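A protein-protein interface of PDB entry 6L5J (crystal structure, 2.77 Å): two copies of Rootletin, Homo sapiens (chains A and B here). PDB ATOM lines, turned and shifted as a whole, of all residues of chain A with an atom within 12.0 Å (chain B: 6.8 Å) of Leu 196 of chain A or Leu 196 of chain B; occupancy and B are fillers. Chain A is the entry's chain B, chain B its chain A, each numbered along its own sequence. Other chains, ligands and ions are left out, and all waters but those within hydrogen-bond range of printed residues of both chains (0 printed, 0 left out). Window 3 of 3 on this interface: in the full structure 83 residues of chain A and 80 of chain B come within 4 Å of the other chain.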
ATOM      1  N   MET A 186      10.471  33.143  -0.015  1.00  0.00           N
ATOM      2  CA  MET A 186       9.943  32.462  -1.197  1.00  0.00           C
ATOM      3  C   MET A 186      10.936  31.424  -1.698  1.00  0.00           C
ATOM      4  O   MET A 186      10.547  30.374  -2.179  1.00  0.00           O
ATOM      5  CB  MET A 186       9.596  33.464  -2.299  1.00  0.00           C
ATOM      6  CG  MET A 186       8.193  34.036  -2.171  1.00  0.00           C
ATOM      7  SD  MET A 186       7.862  35.660  -3.199  1.00  0.00           S
ATOM      8  CE  MET A 186       8.165  35.055  -5.038  1.00  0.00           C
ATOM      9  N   LYS A 187      12.228  31.705  -1.555  1.00  0.00           N
ATOM     10  CA  LYS A 187      13.220  30.756  -2.041  1.00  0.00           C
ATOM     11  C   LYS A 187      13.206  29.472  -1.225  1.00  0.00           C
ATOM     12  O   LYS A 187      13.340  28.384  -1.789  1.00  0.00           O
ATOM     13  CB  LYS A 187      14.599  31.410  -2.045  1.00  0.00           C
ATOM     14  CG  LYS A 187      15.738  30.526  -2.585  1.00  0.00           C
ATOM     15  CD  LYS A 187      16.578  29.921  -1.467  1.00  0.00           C
ATOM     16  CE  LYS A 187      17.595  28.973  -1.985  1.00  0.00           C
ATOM     17  NZ  LYS A 187      17.770  28.208  -0.729  1.00  0.00           N
ATOM     18  N   MET A 188      13.002  29.565   0.088  1.00  0.00           N
ATOM     19  CA  MET A 188      12.950  28.380   0.932  1.00  0.00           C
ATOM     20  C   MET A 188      11.732  27.553   0.588  1.00  0.00           C
ATOM     21  O   MET A 188      11.827  26.376   0.240  1.00  0.00           O
ATOM     22  CB  MET A 188      12.895  28.758   2.402  1.00  0.00           C
ATOM     23  CG  MET A 188      14.118  29.472   2.919  1.00  0.00           C
ATOM     24  SD  MET A 188      13.981  29.922   4.814  1.00  0.00           S
ATOM     25  CE  MET A 188      12.691  31.376   4.706  1.00  0.00           C
ATOM     26  N   LEU A 189      10.575  28.197   0.716  1.00  0.00           N
ATOM     27  CA  LEU A 189       9.316  27.546   0.396  1.00  0.00           C
ATOM     28  C   LEU A 189       9.348  26.937  -0.995  1.00  0.00           C
ATOM     29  O   LEU A 189       8.652  25.950  -1.257  1.00  0.00           O
ATOM     30  CB  LEU A 189       8.177  28.557   0.512  1.00  0.00           C
ATOM     31  CG  LEU A 189       6.789  27.940   0.445  1.00  0.00           C
ATOM     32  CD1 LEU A 189       6.604  27.006   1.629  1.00  0.00           C
ATOM     33  CD2 LEU A 189       5.713  29.010   0.418  1.00  0.00           C
ATOM     34  N   ASP A 190      10.157  27.501  -1.894  1.00  0.00           N
ATOM     35  CA  ASP A 190      10.322  26.931  -3.226  1.00  0.00           C
ATOM     36  C   ASP A 190      11.121  25.639  -3.168  1.00  0.00           C
ATOM     37  O   ASP A 190      10.847  24.697  -3.927  1.00  0.00           O
ATOM     38  CB  ASP A 190      11.006  27.939  -4.138  1.00  0.00           C
ATOM     39  CG  ASP A 190      11.070  27.488  -5.571  1.00  0.00           C
ATOM     40  OD1 ASP A 190      10.017  27.498  -6.241  1.00  0.00           O
ATOM     41  OD2 ASP A 190      12.180  27.152  -6.031  1.00  0.00           O
ATOM     42  N   SER A 191      12.123  25.577  -2.285  1.00  0.00           N
ATOM     43  CA  SER A 191      12.827  24.317  -2.049  1.00  0.00           C
ATOM     44  C   SER A 191      11.935  23.308  -1.332  1.00  0.00           C
ATOM     45  O   SER A 191      12.035  22.100  -1.567  1.00  0.00           O
ATOM     46  CB  SER A 191      14.103  24.564  -1.237  1.00  0.00           C
ATOM     47  OG  SER A 191      15.041  25.336  -1.962  1.00  0.00           O
ATOM     48  N   GLU A 192      11.064  23.789  -0.450  1.00  0.00           N
ATOM     49  CA  GLU A 192      10.134  22.919   0.246  1.00  0.00           C
ATOM     50  C   GLU A 192       9.125  22.291  -0.725  1.00  0.00           C
ATOM     51  O   GLU A 192       8.809  21.094  -0.604  1.00  0.00           O
ATOM     52  CB  GLU A 192       9.466  23.737   1.352  1.00  0.00           C
ATOM     53  CG  GLU A 192       8.574  22.974   2.285  1.00  0.00           C
ATOM     54  CD  GLU A 192       9.314  21.921   3.084  1.00  0.00           C
ATOM     55  OE1 GLU A 192      10.550  22.029   3.267  1.00  0.00           O
ATOM     56  OE2 GLU A 192       8.640  20.982   3.543  1.00  0.00           O
ATOM     57  N   ASN A 193       8.654  23.062  -1.718  1.00  0.00           N
ATOM     58  CA  ASN A 193       7.716  22.530  -2.701  1.00  0.00           C
ATOM     59  C   ASN A 193       8.374  21.480  -3.579  1.00  0.00           C
ATOM     60  O   ASN A 193       7.733  20.496  -3.952  1.00  0.00           O
ATOM     61  CB  ASN A 193       7.141  23.636  -3.590  1.00  0.00           C
ATOM     62  CG  ASN A 193       6.229  24.598  -2.846  1.00  0.00           C
ATOM     63  OD1 ASN A 193       5.485  24.225  -1.937  1.00  0.00           O
ATOM     64  ND2 ASN A 193       6.260  25.852  -3.269  1.00  0.00           N
ATOM     65  N   THR A 194       9.635  21.689  -3.970  1.00  0.00           N
ATOM     66  CA  THR A 194      10.285  20.663  -4.777  1.00  0.00           C
ATOM     67  C   THR A 194      10.652  19.440  -3.938  1.00  0.00           C
ATOM     68  O   THR A 194      10.788  18.334  -4.479  1.00  0.00           O
ATOM     69  CB  THR A 194      11.517  21.225  -5.492  1.00  0.00           C
ATOM     70  OG1 THR A 194      12.094  20.195  -6.308  1.00  0.00           O
ATOM     71  CG2 THR A 194      12.555  21.716  -4.521  1.00  0.00           C
ATOM     72  N   ARG A 195      10.773  19.621  -2.625  1.00  0.00           N
ATOM     73  CA  ARG A 195      10.984  18.497  -1.731  1.00  0.00           C
ATOM     74  C   ARG A 195       9.734  17.620  -1.653  1.00  0.00           C
ATOM     75  O   ARG A 195       9.815  16.387  -1.725  1.00  0.00           O
ATOM     76  CB  ARG A 195      11.352  19.038  -0.359  1.00  0.00           C
ATOM     77  CG  ARG A 195      11.826  17.995   0.569  1.00  0.00           C
ATOM     78  CD  ARG A 195      11.997  18.568   1.940  1.00  0.00           C
ATOM     79  NE  ARG A 195      10.714  18.976   2.504  1.00  0.00           N
ATOM     80  CZ  ARG A 195       9.832  18.123   3.022  1.00  0.00           C
ATOM     81  NH1 ARG A 195      10.086  16.817   3.016  1.00  0.00           N
ATOM     82  NH2 ARG A 195       8.689  18.568   3.531  1.00  0.00           N
ATOM     83  N   LEU A 196       8.571  18.249  -1.490  1.00  0.00           N
ATOM     84  CA  LEU A 196       7.315  17.515  -1.412  1.00  0.00           C
ATOM     85  C   LEU A 196       7.077  16.699  -2.676  1.00  0.00           C
ATOM     86  O   LEU A 196       6.702  15.518  -2.606  1.00  0.00           O
ATOM     87  CB  LEU A 196       6.180  18.512  -1.173  1.00  0.00           C
ATOM     88  CG  LEU A 196       6.247  19.205   0.195  1.00  0.00           C
ATOM     89  CD1 LEU A 196       5.304  20.423   0.345  1.00  0.00           C
ATOM     90  CD2 LEU A 196       5.967  18.147   1.271  1.00  0.00           C
ATOM     91  N   GLY A 197       7.295  17.309  -3.842  1.00  0.00           N
ATOM     92  CA  GLY A 197       7.096  16.588  -5.083  1.00  0.00           C
ATOM     93  C   GLY A 197       8.118  15.506  -5.314  1.00  0.00           C
ATOM     94  O   GLY A 197       7.922  14.661  -6.188  1.00  0.00           O
ATOM     95  N   ARG A 198       9.221  15.540  -4.567  1.00  0.00           N
ATOM     96  CA  ARG A 198      10.154  14.427  -4.546  1.00  0.00           C
ATOM     97  C   ARG A 198       9.606  13.295  -3.689  1.00  0.00           C
ATOM     98  O   ARG A 198       9.795  12.119  -4.020  1.00  0.00           O
ATOM     99  CB  ARG A 198      11.515  14.912  -4.033  1.00  0.00           C
ATOM    100  CG  ARG A 198      12.681  13.955  -4.234  1.00  0.00           C
ATOM    101  CD  ARG A 198      14.000  14.548  -3.721  1.00  0.00           C
ATOM    102  NE  ARG A 198      15.114  13.601  -3.820  1.00  0.00           N
ATOM    103  CZ  ARG A 198      15.939  13.513  -4.860  1.00  0.00           C
ATOM    104  NH1 ARG A 198      15.793  14.334  -5.892  1.00  0.00           N
ATOM    105  NH2 ARG A 198      16.918  12.614  -4.867  1.00  0.00           N
ATOM    106  N   GLU A 199       8.887  13.626  -2.614  1.00  0.00           N
ATOM    107  CA  GLU A 199       8.286  12.574  -1.806  1.00  0.00           C
ATOM    108  C   GLU A 199       7.121  11.887  -2.509  1.00  0.00           C
ATOM    109  O   GLU A 199       6.889  10.701  -2.275  1.00  0.00           O
ATOM    110  CB  GLU A 199       7.852  13.115  -0.450  1.00  0.00           C
ATOM    111  CG  GLU A 199       9.010  13.290   0.500  1.00  0.00           C
ATOM    112  CD  GLU A 199       8.558  13.683   1.881  1.00  0.00           C
ATOM    113  OE1 GLU A 199       7.355  13.978   2.050  1.00  0.00           O
ATOM    114  OE2 GLU A 199       9.401  13.684   2.802  1.00  0.00           O
ATOM    115  N   LEU A 200       6.376  12.587  -3.363  1.00  0.00           N
ATOM    116  CA  LEU A 200       5.374  11.876  -4.144  1.00  0.00           C
ATOM    117  C   LEU A 200       6.014  11.022  -5.220  1.00  0.00           C
ATOM    118  O   LEU A 200       5.465   9.979  -5.588  1.00  0.00           O
ATOM    119  CB  LEU A 200       4.372  12.830  -4.778  1.00  0.00           C
ATOM    120  CG  LEU A 200       3.374  13.469  -3.822  1.00  0.00           C
ATOM    121  CD1 LEU A 200       2.516  14.494  -4.564  1.00  0.00           C
ATOM    122  CD2 LEU A 200       2.509  12.406  -3.136  1.00  0.00           C
ATOM    123  N   ALA A 201       7.172  11.429  -5.726  1.00  0.00           N
ATOM    124  CA  ALA A 201       7.798  10.649  -6.783  1.00  0.00           C
ATOM    125  C   ALA A 201       8.386   9.357  -6.241  1.00  0.00           C
ATOM    126  O   ALA A 201       8.397   8.339  -6.937  1.00  0.00           O
ATOM    127  CB  ALA A 201       8.870  11.473  -7.488  1.00  0.00           C
ATOM    128  N   GLU A 202       8.876   9.374  -5.002  1.00  0.00           N
ATOM    129  CA  GLU A 202       9.411   8.143  -4.436  1.00  0.00           C
ATOM    130  C   GLU A 202       8.293   7.193  -4.028  1.00  0.00           C
ATOM    131  O   GLU A 202       8.392   5.986  -4.261  1.00  0.00           O
ATOM    132  CB  GLU A 202      10.329   8.431  -3.250  1.00  0.00           C
ATOM    133  CG  GLU A 202       9.649   9.041  -2.049  1.00  0.00           C
ATOM    134  CD  GLU A 202      10.577   9.159  -0.855  1.00  0.00           C
ATOM    135  OE1 GLU A 202      11.745   8.728  -0.958  1.00  0.00           O
ATOM    136  OE2 GLU A 202      10.132   9.681   0.191  1.00  0.00           O
ATOM    137  N   LEU A 203       7.212   7.708  -3.439  1.00  0.00           N
ATOM    138  CA  LEU A 203       6.119   6.818  -3.059  1.00  0.00           C
ATOM    139  C   LEU A 203       5.429   6.230  -4.281  1.00  0.00           C
ATOM    140  O   LEU A 203       5.332   5.007  -4.421  1.00  0.00           O
ATOM    141  CB  LEU A 203       5.111   7.547  -2.178  1.00  0.00           C
ATOM    142  CG  LEU A 203       5.645   7.834  -0.789  1.00  0.00           C
ATOM    143  CD1 LEU A 203       4.538   8.443   0.032  1.00  0.00           C
ATOM    144  CD2 LEU A 203       6.167   6.555  -0.163  1.00  0.00           C
ATOM    145  N   GLN A 204       4.944   7.088  -5.181  1.00  0.00           N
ATOM    146  CA  GLN A 204       4.285   6.618  -6.391  1.00  0.00           C
ATOM    147  C   GLN A 204       5.195   5.766  -7.278  1.00  0.00           C
ATOM    148  O   GLN A 204       4.687   5.101  -8.186  1.00  0.00           O
ATOM    149  CB  GLN A 204       3.748   7.822  -7.174  1.00  0.00           C
ATOM    150  CG  GLN A 204       2.592   8.565  -6.489  1.00  0.00           C
ATOM    151  CD  GLN A 204       2.147   9.824  -7.254  1.00  0.00           C
ATOM    152  OE1 GLN A 204       2.756  10.203  -8.254  1.00  0.00           O
ATOM    153  NE2 GLN A 204       1.081  10.465  -6.781  1.00  0.00           N
ATOM    154  N   GLY A 205       6.509   5.756  -7.033  1.00  0.00           N
ATOM    155  CA  GLY A 205       7.446   5.004  -7.851  1.00  0.00           C
ATOM    156  C   GLY A 205       7.924   3.684  -7.263  1.00  0.00           C
ATOM    157  O   GLY A 205       7.940   2.659  -7.952  1.00  0.00           O
ATOM    158  N   ARG A 206       8.343   3.700  -5.997  1.00  0.00           N
ATOM    159  CA  ARG A 206       8.797   2.489  -5.329  1.00  0.00           C
ATOM    160  C   ARG A 206       7.643   1.640  -4.819  1.00  0.00           C
ATOM    161  O   ARG A 206       7.893   0.597  -4.206  1.00  0.00           O
ATOM    162  CB  ARG A 206       9.735   2.834  -4.162  1.00  0.00           C
ATOM    163  CG  ARG A 206       9.049   3.477  -2.979  1.00  0.00           C
ATOM    164  CD  ARG A 206      10.033   3.956  -1.945  1.00  0.00           C
ATOM    165  NE  ARG A 206       9.349   4.678  -0.881  1.00  0.00           N
ATOM    166  CZ  ARG A 206       9.961   5.199   0.175  1.00  0.00           C
ATOM    167  NH1 ARG A 206      11.273   5.066   0.306  1.00  0.00           N
ATOM    168  NH2 ARG A 206       9.264   5.845   1.100  1.00  0.00           N
ATOM    169  N   SER B 191      -0.242  28.338  -1.252  1.00  0.00           N
ATOM    170  CA  SER B 191      -1.360  27.457  -1.593  1.00  0.00           C
ATOM    171  C   SER B 191      -0.849  26.112  -2.075  1.00  0.00           C
ATOM    172  O   SER B 191      -1.301  25.061  -1.616  1.00  0.00           O
ATOM    173  CB  SER B 191      -2.247  28.104  -2.657  1.00  0.00           C
ATOM    174  OG  SER B 191      -3.359  27.287  -2.998  1.00  0.00           O
ATOM    175  N   GLU B 192       0.114  26.141  -2.993  1.00  0.00           N
ATOM    176  CA  GLU B 192       0.723  24.940  -3.534  1.00  0.00           C
ATOM    177  C   GLU B 192       1.485  24.168  -2.463  1.00  0.00           C
ATOM    178  O   GLU B 192       1.620  22.940  -2.554  1.00  0.00           O
ATOM    179  CB  GLU B 192       1.623  25.352  -4.694  1.00  0.00           C
ATOM    180  CG  GLU B 192       2.210  24.255  -5.504  1.00  0.00           C
ATOM    181  CD  GLU B 192       1.156  23.453  -6.248  1.00  0.00           C
ATOM    182  OE1 GLU B 192       0.057  24.019  -6.512  1.00  0.00           O
ATOM    183  OE2 GLU B 192       1.441  22.264  -6.571  1.00  0.00           O
ATOM    184  N   ASN B 193       1.970  24.858  -1.435  1.00  0.00           N
ATOM    185  CA  ASN B 193       2.513  24.188  -0.257  1.00  0.00           C
ATOM    186  C   ASN B 193       1.454  23.312   0.412  1.00  0.00           C
ATOM    187  O   ASN B 193       1.623  22.087   0.523  1.00  0.00           O
ATOM    188  CB  ASN B 193       3.046  25.241   0.719  1.00  0.00           C
ATOM    189  CG  ASN B 193       3.703  24.641   1.958  1.00  0.00           C
ATOM    190  OD1 ASN B 193       3.803  23.417   2.114  1.00  0.00           O
ATOM    191  ND2 ASN B 193       4.127  25.517   2.872  1.00  0.00           N
ATOM    192  N   THR B 194       0.351  23.923   0.864  1.00  0.00           N
ATOM    193  CA  THR B 194      -0.709  23.151   1.494  1.00  0.00           C
ATOM    194  C   THR B 194      -1.306  22.116   0.545  1.00  0.00           C
ATOM    195  O   THR B 194      -1.732  21.043   0.994  1.00  0.00           O
ATOM    196  CB  THR B 194      -1.823  24.054   1.998  1.00  0.00           C
ATOM    197  OG1 THR B 194      -2.427  24.721   0.887  1.00  0.00           O
ATOM    198  CG2 THR B 194      -1.278  25.036   2.973  1.00  0.00           C
ATOM    199  N   ARG B 195      -1.366  22.408  -0.757  1.00  0.00           N
ATOM    200  CA  ARG B 195      -1.960  21.430  -1.648  1.00  0.00           C
ATOM    201  C   ARG B 195      -1.079  20.192  -1.749  1.00  0.00           C
ATOM    202  O   ARG B 195      -1.583  19.064  -1.815  1.00  0.00           O
ATOM    203  CB  ARG B 195      -2.192  21.999  -3.032  1.00  0.00           C
ATOM    204  CG  ARG B 195      -3.045  21.023  -3.832  1.00  0.00           C
ATOM    205  CD  ARG B 195      -3.063  21.354  -5.283  1.00  0.00           C
ATOM    206  NE  ARG B 195      -1.742  21.148  -5.856  1.00  0.00           N
ATOM    207  CZ  ARG B 195      -1.315  19.979  -6.296  1.00  0.00           C
ATOM    208  NH1 ARG B 195      -2.117  18.939  -6.230  1.00  0.00           N
ATOM    209  NH2 ARG B 195      -0.103  19.860  -6.812  1.00  0.00           N
ATOM    210  N   LEU B 196       0.245  20.375  -1.757  1.00  0.00           N
ATOM    211  CA  LEU B 196       1.095  19.195  -1.796  1.00  0.00           C
ATOM    212  C   LEU B 196       0.920  18.341  -0.544  1.00  0.00           C
ATOM    213  O   LEU B 196       0.932  17.110  -0.631  1.00  0.00           O
ATOM    214  CB  LEU B 196       2.557  19.591  -2.012  1.00  0.00           C
ATOM    215  CG  LEU B 196       2.821  20.028  -3.457  1.00  0.00           C
ATOM    216  CD1 LEU B 196       4.308  20.173  -3.732  1.00  0.00           C
ATOM    217  CD2 LEU B 196       2.164  19.065  -4.448  1.00  0.00           C
ATOM    218  N   GLY B 197       0.706  18.972   0.612  1.00  0.00           N
ATOM    219  CA  GLY B 197       0.501  18.205   1.829  1.00  0.00           C
ATOM    220  C   GLY B 197      -0.784  17.397   1.813  1.00  0.00           C
ATOM    221  O   GLY B 197      -0.821  16.264   2.297  1.00  0.00           O
ATOM    222  N   ARG B 198      -1.859  17.972   1.272  1.00  0.00           N
ATOM    223  CA  ARG B 198      -3.106  17.231   1.196  1.00  0.00           C
ATOM    224  C   ARG B 198      -2.981  16.072   0.214  1.00  0.00           C
ATOM    225  O   ARG B 198      -3.500  14.978   0.463  1.00  0.00           O
ATOM    226  CB  ARG B 198      -4.246  18.170   0.808  1.00  0.00           C
ATOM    227  CG  ARG B 198      -4.572  19.191   1.878  1.00  0.00           C
ATOM    228  CD  ARG B 198      -5.604  20.193   1.360  1.00  0.00           C
ATOM    229  NE  ARG B 198      -5.932  21.237   2.328  1.00  0.00           N
ATOM    230  CZ  ARG B 198      -6.799  22.216   2.097  1.00  0.00           C
ATOM    231  NH1 ARG B 198      -7.421  22.291   0.931  1.00  0.00           N
ATOM    232  NH2 ARG B 198      -7.044  23.122   3.034  1.00  0.00           N
ATOM    233  N   GLU B 199      -2.283  16.286  -0.905  1.00  0.00           N
ATOM    234  CA  GLU B 199      -2.051  15.184  -1.824  1.00  0.00           C
ATOM    235  C   GLU B 199      -1.227  14.076  -1.155  1.00  0.00           C
ATOM    236  O   GLU B 199      -1.504  12.889  -1.358  1.00  0.00           O
ATOM    237  CB  GLU B 199      -1.386  15.687  -3.109  1.00  0.00           C
ATOM    238  CG  GLU B 199      -1.261  14.596  -4.133  1.00  0.00           C
ATOM    239  CD  GLU B 199      -0.801  15.023  -5.521  1.00  0.00           C
ATOM    240  OE1 GLU B 199      -0.467  16.200  -5.734  1.00  0.00           O
ATOM    241  OE2 GLU B 199      -0.807  14.143  -6.425  1.00  0.00           O
ATOM    242  N   LEU B 200      -0.258  14.445  -0.313  1.00  0.00           N
ATOM    243  CA  LEU B 200       0.634  13.458   0.288  1.00  0.00           C
ATOM    244  C   LEU B 200      -0.032  12.700   1.440  1.00  0.00           C
ATOM    245  O   LEU B 200       0.066  11.472   1.517  1.00  0.00           O
ATOM    246  CB  LEU B 200       1.918  14.149   0.766  1.00  0.00           C
ATOM    247  CG  LEU B 200       2.996  13.260   1.396  1.00  0.00           C
ATOM    248  CD1 LEU B 200       3.479  12.165   0.426  1.00  0.00           C
ATOM    249  CD2 LEU B 200       4.177  14.086   1.896  1.00  0.00           C
ATOM    250  N   ALA B 201      -0.682  13.421   2.353  1.00  0.00           N
ATOM    251  CA  ALA B 201      -1.378  12.779   3.454  1.00  0.00           C
ATOM    252  C   ALA B 201      -2.491  11.877   2.959  1.00  0.00           C
ATOM    253  O   ALA B 201      -2.697  10.787   3.512  1.00  0.00           O
ATOM    254  CB  ALA B 201      -1.953  13.828   4.394  1.00  0.00           C
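Asn 193 of chain B touches its own counterpart, Asn 193 of chain A. Asn 193 of chain A touches Leu 196 of chain B, and with the chains exchanged Leu 196 of chain A touches Asn 193 of chain B. Leu 196 of chain B touches its own counterpart, Leu 196 of chain A. Leu 200 of chain B touches its own counterpart, Leu 200 of chain A. Positions printed for both chains: 191, 192, 193, 194, 195, 196, 197, 198, 199, 200 and 201. Of the 9 pairs that touch across the chains among the printed residues, 7 have their exchanged pair printed and touching as well.
The guanidinium group of Arg 195 of chain B lies within salt-bridge range of the side-chain carboxylate of Glu 199 of chain B, 3.2 Å away. O of Leu 189 of chain A lies within hydrogen-bond range of ND2 of Asn 193 of chain A, at 3.1 Å. NH1 of Arg 195 of chain A is in salt-bridge range of OE2 of Glu 199 of chain A.
Printed residues of chain B within 4 Å of Leu 196 of chain A: Asn 193 (3.8 Å) and Leu 196 (3.6 Å). Leu 196 of chain B touches just these residues of chain A: Asn 193 (3.4 Å) and Leu 196 (3.6 Å). Printed residues of chain A within 4 Å of Asn 193 of chain B: Leu 189 (3.1 Å), Asn 193 (3.4 Å) and Leu 196 (3.8 Å). Thr 194 of chain B touches none of the printed residues of chain A. Glu 199 of chain B touches just one residue of chain A: Leu 200. Printed residues of chain B within 4 Å of Leu 203 of chain A: Leu 200 (3.9 Å). Of the printed residues of chain B, Glu 199 of chain A touches Leu 200. Of the printed residues of chain B, Leu 200 of chain A touches Glu 199 (3.5 Å) and Leu 200 (3.7 Å). Printed residues of chain B within 4 Å of Leu 189 of chain A: Asn 193 (3.1 Å). Printed residues of chain B within 4 Å of Asn 193 of chain A: Asn 193 and Leu 196. The nearest residue of chain A that does not touch Leu 196 of chain B is Gly 197 of chain A (4.1 Å). The nearest printed residue of chain B that does not touch Leu 203 of chain A is Ala 201 of chain B (7.6 Å).
Printed residues of chain B that touch a printed residue of chain A: Asn 193, Leu 196, Glu 199 and Leu 200. Hydrophobic or aromatic side chains of chain B within 4 Å of the printed part of chain A: Leu 196 and Leu 200. Along chain B the printed residues that touch a printed residue of chain A span positions 193 to 200. Of the 21 printed residues of chain A, 6 touch a printed residue of chain B. Hydrophobic or aromatic side chains of chain A that line the printed part of chain B: Leu 189, Leu 196, Leu 200 and Leu 203. Among the printed residues, 9 pairs touch across the chains. Among the printed residues, no Asp or Glu carboxylate lies within 4 Å of a Lys or Arg side-chain nitrogen of the other chain.
Among the printed residues, pairs that only touch across the chains: Leu 189 of chain A with Asn 193 of chain B, Glu 199 of chain A with Leu 200 of chain B, Asn 193 of chain A with Asn 193 of chain B, Asn 193 of chain A with Leu 196 of chain B, Leu 200 of chain A with Glu 199 of chain B, Leu 196 of chain A with Leu 196 of chain B, Leu 200 of chain A with Leu 200 of chain B, Leu 196 of chain A with Asn 193 of chain B and Leu 203 of chain A with Leu 200 of chain B.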
